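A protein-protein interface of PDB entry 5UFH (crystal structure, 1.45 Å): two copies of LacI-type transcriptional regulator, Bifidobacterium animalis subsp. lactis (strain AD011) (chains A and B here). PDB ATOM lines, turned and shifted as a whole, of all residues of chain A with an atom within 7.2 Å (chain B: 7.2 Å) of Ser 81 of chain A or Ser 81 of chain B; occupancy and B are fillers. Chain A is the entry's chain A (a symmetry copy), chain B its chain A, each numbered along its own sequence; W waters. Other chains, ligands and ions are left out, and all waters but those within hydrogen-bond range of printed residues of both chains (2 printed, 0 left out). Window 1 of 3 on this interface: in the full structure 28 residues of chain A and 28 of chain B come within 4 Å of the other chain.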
ATOM      1  N   ILE A  72     -18.489  31.972   8.969  1.00  0.00           N
ATOM      2  CA  ILE A  72     -19.702  31.653   8.212  1.00  0.00           C
ATOM      3  C   ILE A  72     -20.833  32.574   8.659  1.00  0.00           C
ATOM      4  O   ILE A  72     -20.753  33.260   9.670  1.00  0.00           O
ATOM      5  CB  ILE A  72     -20.151  30.185   8.363  1.00  0.00           C
ATOM      6  CG1 ILE A  72     -20.493  29.932   9.830  1.00  0.00           C
ATOM      7  CG2 ILE A  72     -19.089  29.228   7.866  1.00  0.00           C
ATOM      8  CD1 ILE A  72     -21.412  28.746  10.015  1.00  0.00           C
ATOM      9  N   ASP A  74     -24.285  32.108   9.525  1.00  0.00           N
ATOM     10  CA  ASP A  74     -24.904  31.622  10.761  1.00  0.00           C
ATOM     11  C   ASP A  74     -25.135  30.140  10.546  1.00  0.00           C
ATOM     12  O   ASP A  74     -24.740  29.582   9.520  1.00  0.00           O
ATOM     13  CB  ASP A  74     -26.170  32.381  11.177  1.00  0.00           C
ATOM     14  CG  ASP A  74     -27.341  32.209  10.211  1.00  0.00           C
ATOM     15  OD1 ASP A  74     -27.357  31.270   9.402  1.00  0.00           O
ATOM     16  OD2 ASP A  74     -28.275  33.041  10.285  1.00  0.00           O
ATOM     17  N   PHE A  75     -25.766  29.500  11.510  1.00  0.00           N
ATOM     18  CA  PHE A  75     -26.032  28.067  11.434  1.00  0.00           C
ATOM     19  C   PHE A  75     -27.473  27.753  11.078  1.00  0.00           C
ATOM     20  O   PHE A  75     -27.981  26.667  11.426  1.00  0.00           O
ATOM     21  CB  PHE A  75     -25.647  27.395  12.758  1.00  0.00           C
ATOM     22  CG  PHE A  75     -24.184  27.400  13.008  1.00  0.00           C
ATOM     23  CD1 PHE A  75     -23.374  26.471  12.399  1.00  0.00           C
ATOM     24  CD2 PHE A  75     -23.617  28.367  13.826  1.00  0.00           C
ATOM     25  CE1 PHE A  75     -22.006  26.481  12.610  1.00  0.00           C
ATOM     26  CE2 PHE A  75     -22.256  28.386  14.034  1.00  0.00           C
ATOM     27  CZ  PHE A  75     -21.454  27.443  13.432  1.00  0.00           C
ATOM     28  N   SER A  76     -28.191  28.687  10.466  1.00  0.00           N
ATOM     29  CA  SER A  76     -29.631  28.488  10.369  1.00  0.00           C
ATOM     30  C   SER A  76     -30.016  27.364   9.416  1.00  0.00           C
ATOM     31  O   SER A  76     -31.122  26.820   9.529  1.00  0.00           O
ATOM     32  CB  SER A  76     -30.347  29.774   9.992  1.00  0.00           C
ATOM     33  OG  SER A  76     -29.855  30.282   8.779  1.00  0.00           O
ATOM     34  N   GLN A  77     -29.146  26.990   8.506  1.00  0.00           N
ATOM     35  CA  GLN A  77     -29.476  25.929   7.576  1.00  0.00           C
ATOM     36  C   GLN A  77     -28.450  24.811   7.689  1.00  0.00           C
ATOM     37  O   GLN A  77     -27.292  25.047   8.056  1.00  0.00           O
ATOM     38  CB  GLN A  77     -29.538  26.447   6.135  1.00  0.00           C
ATOM     39  CG  GLN A  77     -30.506  27.624   5.920  1.00  0.00           C
ATOM     40  CD  GLN A  77     -31.840  27.451   6.618  1.00  0.00           C
ATOM     41  OE1 GLN A  77     -32.565  26.472   6.394  1.00  0.00           O
ATOM     42  NE2 GLN A  77     -32.178  28.414   7.476  1.00  0.00           N
ATOM     43  N   PRO A  78     -28.873  23.573   7.418  1.00  0.00           N
ATOM     44  CA  PRO A  78     -28.016  22.409   7.702  1.00  0.00           C
ATOM     45  C   PRO A  78     -26.649  22.431   7.051  1.00  0.00           C
ATOM     46  O   PRO A  78     -25.689  21.870   7.608  1.00  0.00           O
ATOM     47  CB  PRO A  78     -28.883  21.226   7.240  1.00  0.00           C
ATOM     48  CG  PRO A  78     -30.281  21.715   7.274  1.00  0.00           C
ATOM     49  CD  PRO A  78     -30.213  23.192   6.965  1.00  0.00           C
ATOM     50  N   PHE A  79     -26.473  23.069   5.885  1.00  0.00           N
ATOM     51  CA  PHE A  79     -25.188  23.004   5.235  1.00  0.00           C
ATOM     52  C   PHE A  79     -24.069  23.607   6.093  1.00  0.00           C
ATOM     53  O   PHE A  79     -22.947  23.094   6.104  1.00  0.00           O
ATOM     54  CB  PHE A  79     -25.265  23.727   3.885  1.00  0.00           C
ATOM     55  CG  PHE A  79     -23.939  23.856   3.232  1.00  0.00           C
ATOM     56  CD1 PHE A  79     -23.361  22.778   2.546  1.00  0.00           C
ATOM     57  CD2 PHE A  79     -23.226  25.045   3.312  1.00  0.00           C
ATOM     58  CE1 PHE A  79     -22.087  22.908   1.950  1.00  0.00           C
ATOM     59  CE2 PHE A  79     -22.002  25.177   2.756  1.00  0.00           C
ATOM     60  CZ  PHE A  79     -21.418  24.109   2.064  1.00  0.00           C
ATOM     61  N   ALA A  80     -24.366  24.677   6.848  1.00  0.00           N
ATOM     62  CA  ALA A  80     -23.286  25.318   7.601  1.00  0.00           C
ATOM     63  C   ALA A  80     -22.715  24.356   8.652  1.00  0.00           C
ATOM     64  O   ALA A  80     -21.488  24.264   8.805  1.00  0.00           O
ATOM     65  CB  ALA A  80     -23.825  26.579   8.292  1.00  0.00           C
ATOM     66  N   SER A  81     -23.601  23.622   9.337  1.00  0.00           N
ATOM     67  CA  SER A  81     -23.198  22.588  10.294  1.00  0.00           C
ATOM     68  C   SER A  81     -22.356  21.532   9.616  1.00  0.00           C
ATOM     69  O   SER A  81     -21.324  21.099  10.138  1.00  0.00           O
ATOM     70  CB  SER A  81     -24.448  21.882  10.866  1.00  0.00           C
ATOM     71  OG  SER A  81     -25.117  22.685  11.801  1.00  0.00           O
ATOM     72  N   TYR A  82     -22.818  21.062   8.466  1.00  0.00           N
ATOM     73  CA  TYR A  82     -22.147  19.954   7.816  1.00  0.00           C
ATOM     74  C   TYR A  82     -20.762  20.379   7.341  1.00  0.00           C
ATOM     75  O   TYR A  82     -19.771  19.662   7.551  1.00  0.00           O
ATOM     76  CB  TYR A  82     -23.054  19.520   6.659  1.00  0.00           C
ATOM     77  CG  TYR A  82     -22.558  18.352   5.862  1.00  0.00           C
ATOM     78  CD1 TYR A  82     -22.133  17.187   6.495  1.00  0.00           C
ATOM     79  CD2 TYR A  82     -22.579  18.385   4.474  1.00  0.00           C
ATOM     80  CE1 TYR A  82     -21.696  16.101   5.761  1.00  0.00           C
ATOM     81  CE2 TYR A  82     -22.141  17.299   3.727  1.00  0.00           C
ATOM     82  CZ  TYR A  82     -21.702  16.164   4.381  1.00  0.00           C
ATOM     83  OH  TYR A  82     -21.272  15.080   3.652  1.00  0.00           O
ATOM     84  N   LEU A  83     -20.655  21.566   6.742  1.00  0.00           N
ATOM     85  CA  LEU A  83     -19.356  22.045   6.294  1.00  0.00           C
ATOM     86  C   LEU A  83     -18.421  22.263   7.473  1.00  0.00           C
ATOM     87  O   LEU A  83     -17.262  21.840   7.441  1.00  0.00           O
ATOM     88  CB  LEU A  83     -19.515  23.338   5.469  1.00  0.00           C
ATOM     89  CG  LEU A  83     -18.219  23.998   5.007  1.00  0.00           C
ATOM     90  CD1 LEU A  83     -17.374  23.111   4.045  1.00  0.00           C
ATOM     91  CD2 LEU A  83     -18.495  25.382   4.385  1.00  0.00           C
ATOM     92  N   ALA A  84     -18.918  22.905   8.533  1.00  0.00           N
ATOM     93  CA  ALA A  84     -18.071  23.137   9.697  1.00  0.00           C
ATOM     94  C   ALA A  84     -17.555  21.823  10.268  1.00  0.00           C
ATOM     95  O   ALA A  84     -16.364  21.705  10.609  1.00  0.00           O
ATOM     96  CB  ALA A  84     -18.846  23.911  10.780  1.00  0.00           C
ATOM     97  N   ASP A  85     -18.443  20.841  10.429  1.00  0.00           N
ATOM     98  CA  ASP A  85     -17.995  19.562  10.991  1.00  0.00           C
ATOM     99  C   ASP A  85     -16.923  18.929  10.106  1.00  0.00           C
ATOM    100  O   ASP A  85     -15.947  18.378  10.617  1.00  0.00           O
ATOM    101  CB  ASP A  85     -19.158  18.593  11.189  1.00  0.00           C
ATOM    102  CG  ASP A  85     -19.989  18.915  12.422  1.00  0.00           C
ATOM    103  OD1 ASP A  85     -19.514  19.650  13.325  1.00  0.00           O
ATOM    104  OD2 ASP A  85     -21.133  18.414  12.475  1.00  0.00           O
ATOM    105  N   GLN A  86     -17.083  18.998   8.780  1.00  0.00           N
ATOM    106  CA  GLN A  86     -16.079  18.395   7.910  1.00  0.00           C
ATOM    107  C   GLN A  86     -14.750  19.139   7.994  1.00  0.00           C
ATOM    108  O   GLN A  86     -13.691  18.513   8.044  1.00  0.00           O
ATOM    109  CB  GLN A  86     -16.604  18.336   6.485  1.00  0.00           C
ATOM    110  CG  GLN A  86     -17.721  17.297   6.300  1.00  0.00           C
ATOM    111  CD  GLN A  86     -17.205  15.858   6.433  1.00  0.00           C
ATOM    112  OE1 GLN A  86     -16.060  15.554   6.063  1.00  0.00           O
ATOM    113  NE2 GLN A  86     -18.040  14.975   6.966  1.00  0.00           N
ATOM    114  N   ILE A  87     -14.785  20.471   8.051  1.00  0.00           N
ATOM    115  CA  ILE A  87     -13.563  21.238   8.267  1.00  0.00           C
ATOM    116  C   ILE A  87     -12.894  20.852   9.575  1.00  0.00           C
ATOM    117  O   ILE A  87     -11.670  20.680   9.631  1.00  0.00           O
ATOM    118  CB  ILE A  87     -13.850  22.743   8.135  1.00  0.00           C
ATOM    119  CG1 ILE A  87     -14.091  23.056   6.641  1.00  0.00           C
ATOM    120  CG2 ILE A  87     -12.717  23.566   8.731  1.00  0.00           C
ATOM    121  CD1 ILE A  87     -14.588  24.474   6.387  1.00  0.00           C
ATOM    122  N   ILE A  88     -13.685  20.680  10.646  1.00  0.00           N
ATOM    123  CA  ILE A  88     -13.122  20.268  11.931  1.00  0.00           C
ATOM    124  C   ILE A  88     -12.439  18.908  11.829  1.00  0.00           C
ATOM    125  O   ILE A  88     -11.326  18.724  12.332  1.00  0.00           O
ATOM    126  CB  ILE A  88     -14.192  20.306  13.041  1.00  0.00           C
ATOM    127  CG1 ILE A  88     -14.631  21.749  13.264  1.00  0.00           C
ATOM    128  CG2 ILE A  88     -13.684  19.665  14.367  1.00  0.00           C
ATOM    129  CD1 ILE A  88     -16.011  21.845  13.899  1.00  0.00           C
ATOM    130  N   PRO A 292     -26.724  15.559   5.638  1.00  0.00           N
ATOM    131  CA  PRO A 292     -27.293  14.374   6.306  1.00  0.00           C
ATOM    132  C   PRO A 292     -28.813  14.305   6.319  1.00  0.00           C
ATOM    133  O   PRO A 292     -29.368  13.223   6.099  1.00  0.00           O
ATOM    134  CB  PRO A 292     -26.651  14.431   7.704  1.00  0.00           C
ATOM    135  CG  PRO A 292     -25.281  15.004   7.437  1.00  0.00           C
ATOM    136  CD  PRO A 292     -25.530  16.070   6.345  1.00  0.00           C
ATOM    137  N   GLU A 293     -29.492  15.439   6.528  1.00  0.00           N
ATOM    138  CA  GLU A 293     -30.946  15.467   6.569  1.00  0.00           C
ATOM    139  C   GLU A 293     -31.579  14.817   5.348  1.00  0.00           C
ATOM    140  O   GLU A 293     -32.654  14.224   5.460  1.00  0.00           O
ATOM    141  CB  GLU A 293     -31.445  16.908   6.665  1.00  0.00           C
ATOM    142  CG  GLU A 293     -31.319  17.507   8.038  1.00  0.00           C
ATOM    143  CD  GLU A 293     -29.893  17.923   8.428  1.00  0.00           C
ATOM    144  OE1 GLU A 293     -28.898  17.720   7.703  1.00  0.00           O
ATOM    145  OE2 GLU A 293     -29.786  18.478   9.548  1.00  0.00           O
ATOM    146  N   ILE B  72     -19.094  23.655  22.387  1.00  0.00           N
ATOM    147  CA  ILE B  72     -20.052  22.567  22.174  1.00  0.00           C
ATOM    148  C   ILE B  72     -19.334  21.378  21.542  1.00  0.00           C
ATOM    149  O   ILE B  72     -18.209  21.473  21.070  1.00  0.00           O
ATOM    150  CB  ILE B  72     -21.249  22.968  21.288  1.00  0.00           C
ATOM    151  CG1 ILE B  72     -20.723  23.341  19.904  1.00  0.00           C
ATOM    152  CG2 ILE B  72     -22.040  24.101  21.906  1.00  0.00           C
ATOM    153  CD1 ILE B  72     -21.785  23.243  18.833  1.00  0.00           C
ATOM    154  N   ASP B  74     -20.041  19.150  18.818  1.00  0.00           N
ATOM    155  CA  ASP B  74     -19.893  19.330  17.372  1.00  0.00           C
ATOM    156  C   ASP B  74     -21.253  19.782  16.877  1.00  0.00           C
ATOM    157  O   ASP B  74     -22.172  20.001  17.669  1.00  0.00           O
ATOM    158  CB  ASP B  74     -19.355  18.100  16.631  1.00  0.00           C
ATOM    159  CG  ASP B  74     -20.301  16.901  16.651  1.00  0.00           C
ATOM    160  OD1 ASP B  74     -21.502  17.051  16.917  1.00  0.00           O
ATOM    161  OD2 ASP B  74     -19.814  15.780  16.378  1.00  0.00           O
ATOM    162  N   PHE B  75     -21.381  19.930  15.573  1.00  0.00           N
ATOM    163  CA  PHE B  75     -22.632  20.380  14.972  1.00  0.00           C
ATOM    164  C   PHE B  75     -23.419  19.251  14.332  1.00  0.00           C
ATOM    165  O   PHE B  75     -24.215  19.492  13.401  1.00  0.00           O
ATOM    166  CB  PHE B  75     -22.349  21.485  13.946  1.00  0.00           C
ATOM    167  CG  PHE B  75     -21.863  22.743  14.567  1.00  0.00           C
ATOM    168  CD1 PHE B  75     -22.753  23.621  15.140  1.00  0.00           C
ATOM    169  CD2 PHE B  75     -20.505  23.023  14.609  1.00  0.00           C
ATOM    170  CE1 PHE B  75     -22.306  24.786  15.740  1.00  0.00           C
ATOM    171  CE2 PHE B  75     -20.054  24.177  15.210  1.00  0.00           C
ATOM    172  CZ  PHE B  75     -20.953  25.058  15.769  1.00  0.00           C
ATOM    173  N   SER B  76     -23.178  18.008  14.732  1.00  0.00           N
ATOM    174  CA  SER B  76     -23.729  16.918  13.939  1.00  0.00           C
ATOM    175  C   SER B  76     -25.245  16.809  14.043  1.00  0.00           C
ATOM    176  O   SER B  76     -25.878  16.227  13.153  1.00  0.00           O
ATOM    177  CB  SER B  76     -23.077  15.590  14.287  1.00  0.00           C
ATOM    178  OG  SER B  76     -23.223  15.305  15.655  1.00  0.00           O
ATOM    179  N   GLN B  77     -25.842  17.360  15.075  1.00  0.00           N
ATOM    180  CA  GLN B  77     -27.282  17.275  15.215  1.00  0.00           C
ATOM    181  C   GLN B  77     -27.873  18.675  15.296  1.00  0.00           C
ATOM    182  O   GLN B  77     -27.209  19.619  15.742  1.00  0.00           O
ATOM    183  CB  GLN B  77     -27.677  16.461  16.451  1.00  0.00           C
ATOM    184  CG  GLN B  77     -27.081  15.042  16.500  1.00  0.00           C
ATOM    185  CD  GLN B  77     -27.148  14.308  15.177  1.00  0.00           C
ATOM    186  OE1 GLN B  77     -28.226  14.119  14.595  1.00  0.00           O
ATOM    187  NE2 GLN B  77     -25.984  13.881  14.688  1.00  0.00           N
ATOM    188  N   PRO B  78     -29.112  18.836  14.824  1.00  0.00           N
ATOM    189  CA  PRO B  78     -29.685  20.184  14.667  1.00  0.00           C
ATOM    190  C   PRO B  78     -29.705  21.034  15.920  1.00  0.00           C
ATOM    191  O   PRO B  78     -29.621  22.272  15.829  1.00  0.00           O
ATOM    192  CB  PRO B  78     -31.091  19.895  14.114  1.00  0.00           C
ATOM    193  CG  PRO B  78     -31.010  18.552  13.492  1.00  0.00           C
ATOM    194  CD  PRO B  78     -29.982  17.785  14.290  1.00  0.00           C
ATOM    195  N   PHE B  79     -29.797  20.451  17.123  1.00  0.00           N
ATOM    196  CA  PHE B  79     -29.906  21.278  18.299  1.00  0.00           C
ATOM    197  C   PHE B  79     -28.686  22.190  18.485  1.00  0.00           C
ATOM    198  O   PHE B  79     -28.827  23.339  18.912  1.00  0.00           O
ATOM    199  CB  PHE B  79     -30.090  20.386  19.532  1.00  0.00           C
ATOM    200  CG  PHE B  79     -30.035  21.151  20.802  1.00  0.00           C
ATOM    201  CD1 PHE B  79     -31.140  21.888  21.252  1.00  0.00           C
ATOM    202  CD2 PHE B  79     -28.872  21.178  21.560  1.00  0.00           C
ATOM    203  CE1 PHE B  79     -31.066  22.632  22.451  1.00  0.00           C
ATOM    204  CE2 PHE B  79     -28.785  21.896  22.702  1.00  0.00           C
ATOM    205  CZ  PHE B  79     -29.884  22.629  23.163  1.00  0.00           C
ATOM    206  N   ALA B  80     -27.483  21.707  18.135  1.00  0.00           N
ATOM    207  CA  ALA B  80     -26.302  22.531  18.392  1.00  0.00           C
ATOM    208  C   ALA B  80     -26.357  23.827  17.571  1.00  0.00           C
ATOM    209  O   ALA B  80     -26.057  24.909  18.101  1.00  0.00           O
ATOM    210  CB  ALA B  80     -25.038  21.740  18.024  1.00  0.00           C
ATOM    211  N   SER B  81     -26.774  23.717  16.304  1.00  0.00           N
ATOM    212  CA  SER B  81     -26.979  24.879  15.436  1.00  0.00           C
ATOM    213  C   SER B  81     -28.000  25.819  16.033  1.00  0.00           C
ATOM    214  O   SER B  81     -27.816  27.040  16.055  1.00  0.00           O
ATOM    215  CB  SER B  81     -27.522  24.423  14.063  1.00  0.00           C
ATOM    216  OG  SER B  81     -26.522  23.836  13.276  1.00  0.00           O
ATOM    217  N   TYR B  82     -29.120  25.265  16.478  1.00  0.00           N
ATOM    218  CA  TYR B  82     -30.207  26.103  16.941  1.00  0.00           C
ATOM    219  C   TYR B  82     -29.803  26.837  18.215  1.00  0.00           C
ATOM    220  O   TYR B  82     -30.028  28.050  18.348  1.00  0.00           O
ATOM    221  CB  TYR B  82     -31.406  25.172  17.158  1.00  0.00           C
ATOM    222  CG  TYR B  82     -32.663  25.848  17.615  1.00  0.00           C
ATOM    223  CD1 TYR B  82     -33.146  26.975  16.956  1.00  0.00           C
ATOM    224  CD2 TYR B  82     -33.408  25.318  18.661  1.00  0.00           C
ATOM    225  CE1 TYR B  82     -34.317  27.585  17.362  1.00  0.00           C
ATOM    226  CE2 TYR B  82     -34.587  25.925  19.077  1.00  0.00           C
ATOM    227  CZ  TYR B  82     -35.031  27.057  18.421  1.00  0.00           C
ATOM    228  OH  TYR B  82     -36.199  27.662  18.820  1.00  0.00           O
ATOM    229  N   LEU B  83     -29.159  26.137  19.150  1.00  0.00           N
ATOM    230  CA  LEU B  83     -28.717  26.786  20.376  1.00  0.00           C
ATOM    231  C   LEU B  83     -27.672  27.850  20.081  1.00  0.00           C
ATOM    232  O   LEU B  83     -27.756  28.970  20.593  1.00  0.00           O
ATOM    233  CB  LEU B  83     -28.176  25.740  21.372  1.00  0.00           C
ATOM    234  CG  LEU B  83     -27.597  26.295  22.671  1.00  0.00           C
ATOM    235  CD1 LEU B  83     -28.639  27.054  23.545  1.00  0.00           C
ATOM    236  CD2 LEU B  83     -26.898  25.185  23.482  1.00  0.00           C
ATOM    237  N   ALA B  84     -26.690  27.522  19.237  1.00  0.00           N
ATOM    238  CA  ALA B  84     -25.664  28.504  18.911  1.00  0.00           C
ATOM    239  C   ALA B  84     -26.279  29.754  18.296  1.00  0.00           C
ATOM    240  O   ALA B  84     -25.905  30.886  18.653  1.00  0.00           O
ATOM    241  CB  ALA B  84     -24.629  27.898  17.944  1.00  0.00           C
ATOM    242  N   ASP B  85     -27.185  29.573  17.333  1.00  0.00           N
ATOM    243  CA  ASP B  85     -27.793  30.749  16.700  1.00  0.00           C
ATOM    244  C   ASP B  85     -28.536  31.595  17.731  1.00  0.00           C
ATOM    245  O   ASP B  85     -28.465  32.824  17.688  1.00  0.00           O
ATOM    246  CB  ASP B  85     -28.732  30.356  15.562  1.00  0.00           C
ATOM    247  CG  ASP B  85     -27.989  29.976  14.290  1.00  0.00           C
ATOM    248  OD1 ASP B  85     -26.792  30.325  14.134  1.00  0.00           O
ATOM    249  OD2 ASP B  85     -28.630  29.321  13.440  1.00  0.00           O
ATOM    250  N   GLN B  86     -29.249  30.960  18.667  1.00  0.00           N
ATOM    251  CA  GLN B  86     -29.975  31.743  19.661  1.00  0.00           C
ATOM    252  C   GLN B  86     -29.021  32.478  20.598  1.00  0.00           C
ATOM    253  O   GLN B  86     -29.246  33.645  20.920  1.00  0.00           O
ATOM    254  CB  GLN B  86     -30.933  30.842  20.424  1.00  0.00           C
ATOM    255  CG  GLN B  86     -32.129  30.382  19.576  1.00  0.00           C
ATOM    256  CD  GLN B  86     -33.086  31.536  19.246  1.00  0.00           C
ATOM    257  OE1 GLN B  86     -33.264  32.466  20.048  1.00  0.00           O
ATOM    258  NE2 GLN B  86     -33.694  31.483  18.068  1.00  0.00           N
ATOM    259  N   ILE B  87     -27.932  31.829  21.011  1.00  0.00           N
ATOM    260  CA  ILE B  87     -26.912  32.515  21.797  1.00  0.00           C
ATOM    261  C   ILE B  87     -26.342  33.703  21.042  1.00  0.00           C
ATOM    262  O   ILE B  87     -26.161  34.785  21.614  1.00  0.00           O
ATOM    263  CB  ILE B  87     -25.848  31.513  22.276  1.00  0.00           C
ATOM    264  CG1 ILE B  87     -26.478  30.636  23.380  1.00  0.00           C
ATOM    265  CG2 ILE B  87     -24.594  32.236  22.746  1.00  0.00           C
ATOM    266  CD1 ILE B  87     -25.601  29.464  23.804  1.00  0.00           C
ATOM    267  N   ILE B  88     -26.075  33.536  19.737  1.00  0.00           N
ATOM    268  CA  ILE B  88     -25.563  34.645  18.932  1.00  0.00           C
ATOM    269  C   ILE B  88     -26.547  35.809  18.900  1.00  0.00           C
ATOM    270  O   ILE B  88     -26.155  36.968  19.069  1.00  0.00           O
ATOM    271  CB  ILE B  88     -25.172  34.167  17.519  1.00  0.00           C
ATOM    272  CG1 ILE B  88     -23.997  33.200  17.625  1.00  0.00           C
ATOM    273  CG2 ILE B  88     -24.834  35.356  16.571  1.00  0.00           C
ATOM    274  CD1 ILE B  88     -23.895  32.276  16.419  1.00  0.00           C
ATOM    275  N   PRO B 292     -36.002  23.778  14.487  1.00  0.00           N
ATOM    276  CA  PRO B 292     -36.715  24.133  13.245  1.00  0.00           C
ATOM    277  C   PRO B 292     -37.121  22.954  12.373  1.00  0.00           C
ATOM    278  O   PRO B 292     -38.238  22.953  11.846  1.00  0.00           O
ATOM    279  CB  PRO B 292     -35.748  25.119  12.567  1.00  0.00           C
ATOM    280  CG  PRO B 292     -35.114  25.843  13.729  1.00  0.00           C
ATOM    281  CD  PRO B 292     -34.922  24.741  14.796  1.00  0.00           C
ATOM    282  N   GLU B 293     -36.258  21.939  12.246  1.00  0.00           N
ATOM    283  CA  GLU B 293     -36.555  20.778  11.423  1.00  0.00           C
ATOM    284  C   GLU B 293     -37.897  20.147  11.761  1.00  0.00           C
ATOM    285  O   GLU B 293     -38.562  19.613  10.872  1.00  0.00           O
ATOM    286  CB  GLU B 293     -35.466  19.718  11.590  1.00  0.00           C
ATOM    287  CG  GLU B 293     -34.200  20.022  10.840  1.00  0.00           C
ATOM    288  CD  GLU B 293     -33.316  21.102  11.481  1.00  0.00           C
ATOM    289  OE1 GLU B 293     -33.644  21.737  12.503  1.00  0.00           O
ATOM    290  OE2 GLU B 293     -32.229  21.320  10.894  1.00  0.00           O
HETATM  291  O   HOH W   1     -26.399  24.406  10.498  1.00  0.00           O
HETATM  292  O   HOH W   2     -26.164  21.515  14.166  1.00  0.00           O
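Asp 74 of chain A touches Asp 85 of chain B, and with the chains exchanged Asp 85 of chain A touches Asp 74 of chain B. Phe 75 of chain A touches its own counterpart, Phe 75 of chain B. Phe 75 of chain A touches Ser 81 of chain B, and with the chains exchanged Ser 81 of chain A touches Phe 75 of chain B. Ser 76 of chain A touches Asp 85 of chain B, and with the chains exchanged Asp 85 of chain A touches Ser 76 of chain B. 18 positions are printed for both chains.
Water W2 lies within hydrogen-bond range of the side-chain hydroxyl of Ser 81 of chain B (2.5 Å), the backbone carbonyl oxygen of Gln 77 of chain B (2.7 Å), the side-chain hydroxyl of Ser 81 of chain A (2.8 Å) and the backbone carbonyl oxygen of Phe 75 of chain B (2.9 Å). Water W1 lies within hydrogen-bond range of the side-chain hydroxyl (OG) of Ser 81 of chain A (2.5 Å), the backbone carbonyl oxygen (O) of Gln 77 of chain A (2.7 Å), the side-chain hydroxyl (OG) of Ser 81 of chain B (2.8 Å) and the backbone carbonyl oxygen (O) of Phe 75 of chain A (2.9 Å).
The backbone NH of Phe 75 of chain A is in hydrogen-bond range of the side-chain carboxylate of Asp 85 of chain B, 2.9 Å away. The backbone NH (N) of Phe 75 of chain B sits at hydrogen-bond distance from the side-chain carboxylate (OD1) of Asp 85 of chain A (2.9 Å). The side-chain carboxylate (OD2) of Asp 85 of chain B is in hydrogen-bond range of the backbone NH (N) of Ser 76 of chain A (3.1 Å). The side-chain hydroxyl (OG) of Ser 81 of chain A lies close to the side-chain hydroxyl (OG) of Ser 81 of chain B (2.3 Å). The backbone NH (N) of Ser 76 of chain B lies within hydrogen-bond range of the side-chain carboxylate (OD2) of Asp 85 of chain A, 3.1 Å away.
Hydrophobic or aromatic side chains of chain B within 4 Å of the printed part of chain A: Phe 75. Among the printed residues, no Asp or Glu carboxylate lies within 4 Å of a Lys or Arg side-chain nitrogen of the other chain.
Of the printed residues of chain B, Ser 76 of chain A touches Asp 85 (3.1 Å). No residue of chain B comes within 4 Å of Ala 80 of chain A. Of the printed residues of chain B, Ser 81 of chain A touches Phe 75 (3.5 Å) and Ser 81 (2.3 Å). Tyr 82 of chain A touches none of the printed residues of chain B. Ile 87 of chain A touches none of the printed residues of chain B. Of the printed residues of chain A, Phe 75 of chain B touches Phe 75 (3.4 Å), Ser 81 (3.5 Å) and Asp 85 (2.9 Å). Of the printed residues of chain A, Ser 76 of chain B touches Asp 85. No residue of chain A comes within 4 Å of Ala 80 of chain B. Ser 81 of chain B touches just these residues of chain A: Phe 75 and Ser 81. The nearest residue of chain B that does not touch Ser 81 of chain A is Gln 77 of chain B (5.4 Å).
OD1 of Asp 74 of chain A is in hydrogen-bond range of OG of Ser 76 of chain A (2.8 Å). The side-chain hydroxyl (OG) of Ser 76 of chain B sits close to the side-chain amide nitrogen (NE2) of Gln 77 of chain B (3.3 Å). The side-chain hydroxyl (OG) of Ser 76 of chain B is in hydrogen-bond range of the side-chain carboxylate (OD1) of Asp 74 of chain B. The side-chain hydroxyl of Ser 76 of chain A sits close to the side-chain amide nitrogen of Gln 77 of chain A.
CB of Asp 74 of chain A touches OD1 of Asp 85 of chain B, 3.7 Å away. Phe 75 of chain B touches Phe 75 of chain A. Ser 81 of chain B touches Phe 75 of chain A. Ser 81 of chain A touches Phe 75 of chain B. CB of Asp 74 of chain B touches OD1 of Asp 85 of chain A, at 3.7 Å. OE2 of Glu 293 of chain A touches OE2 of Glu 293 of chain B, 3.98 Å away.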
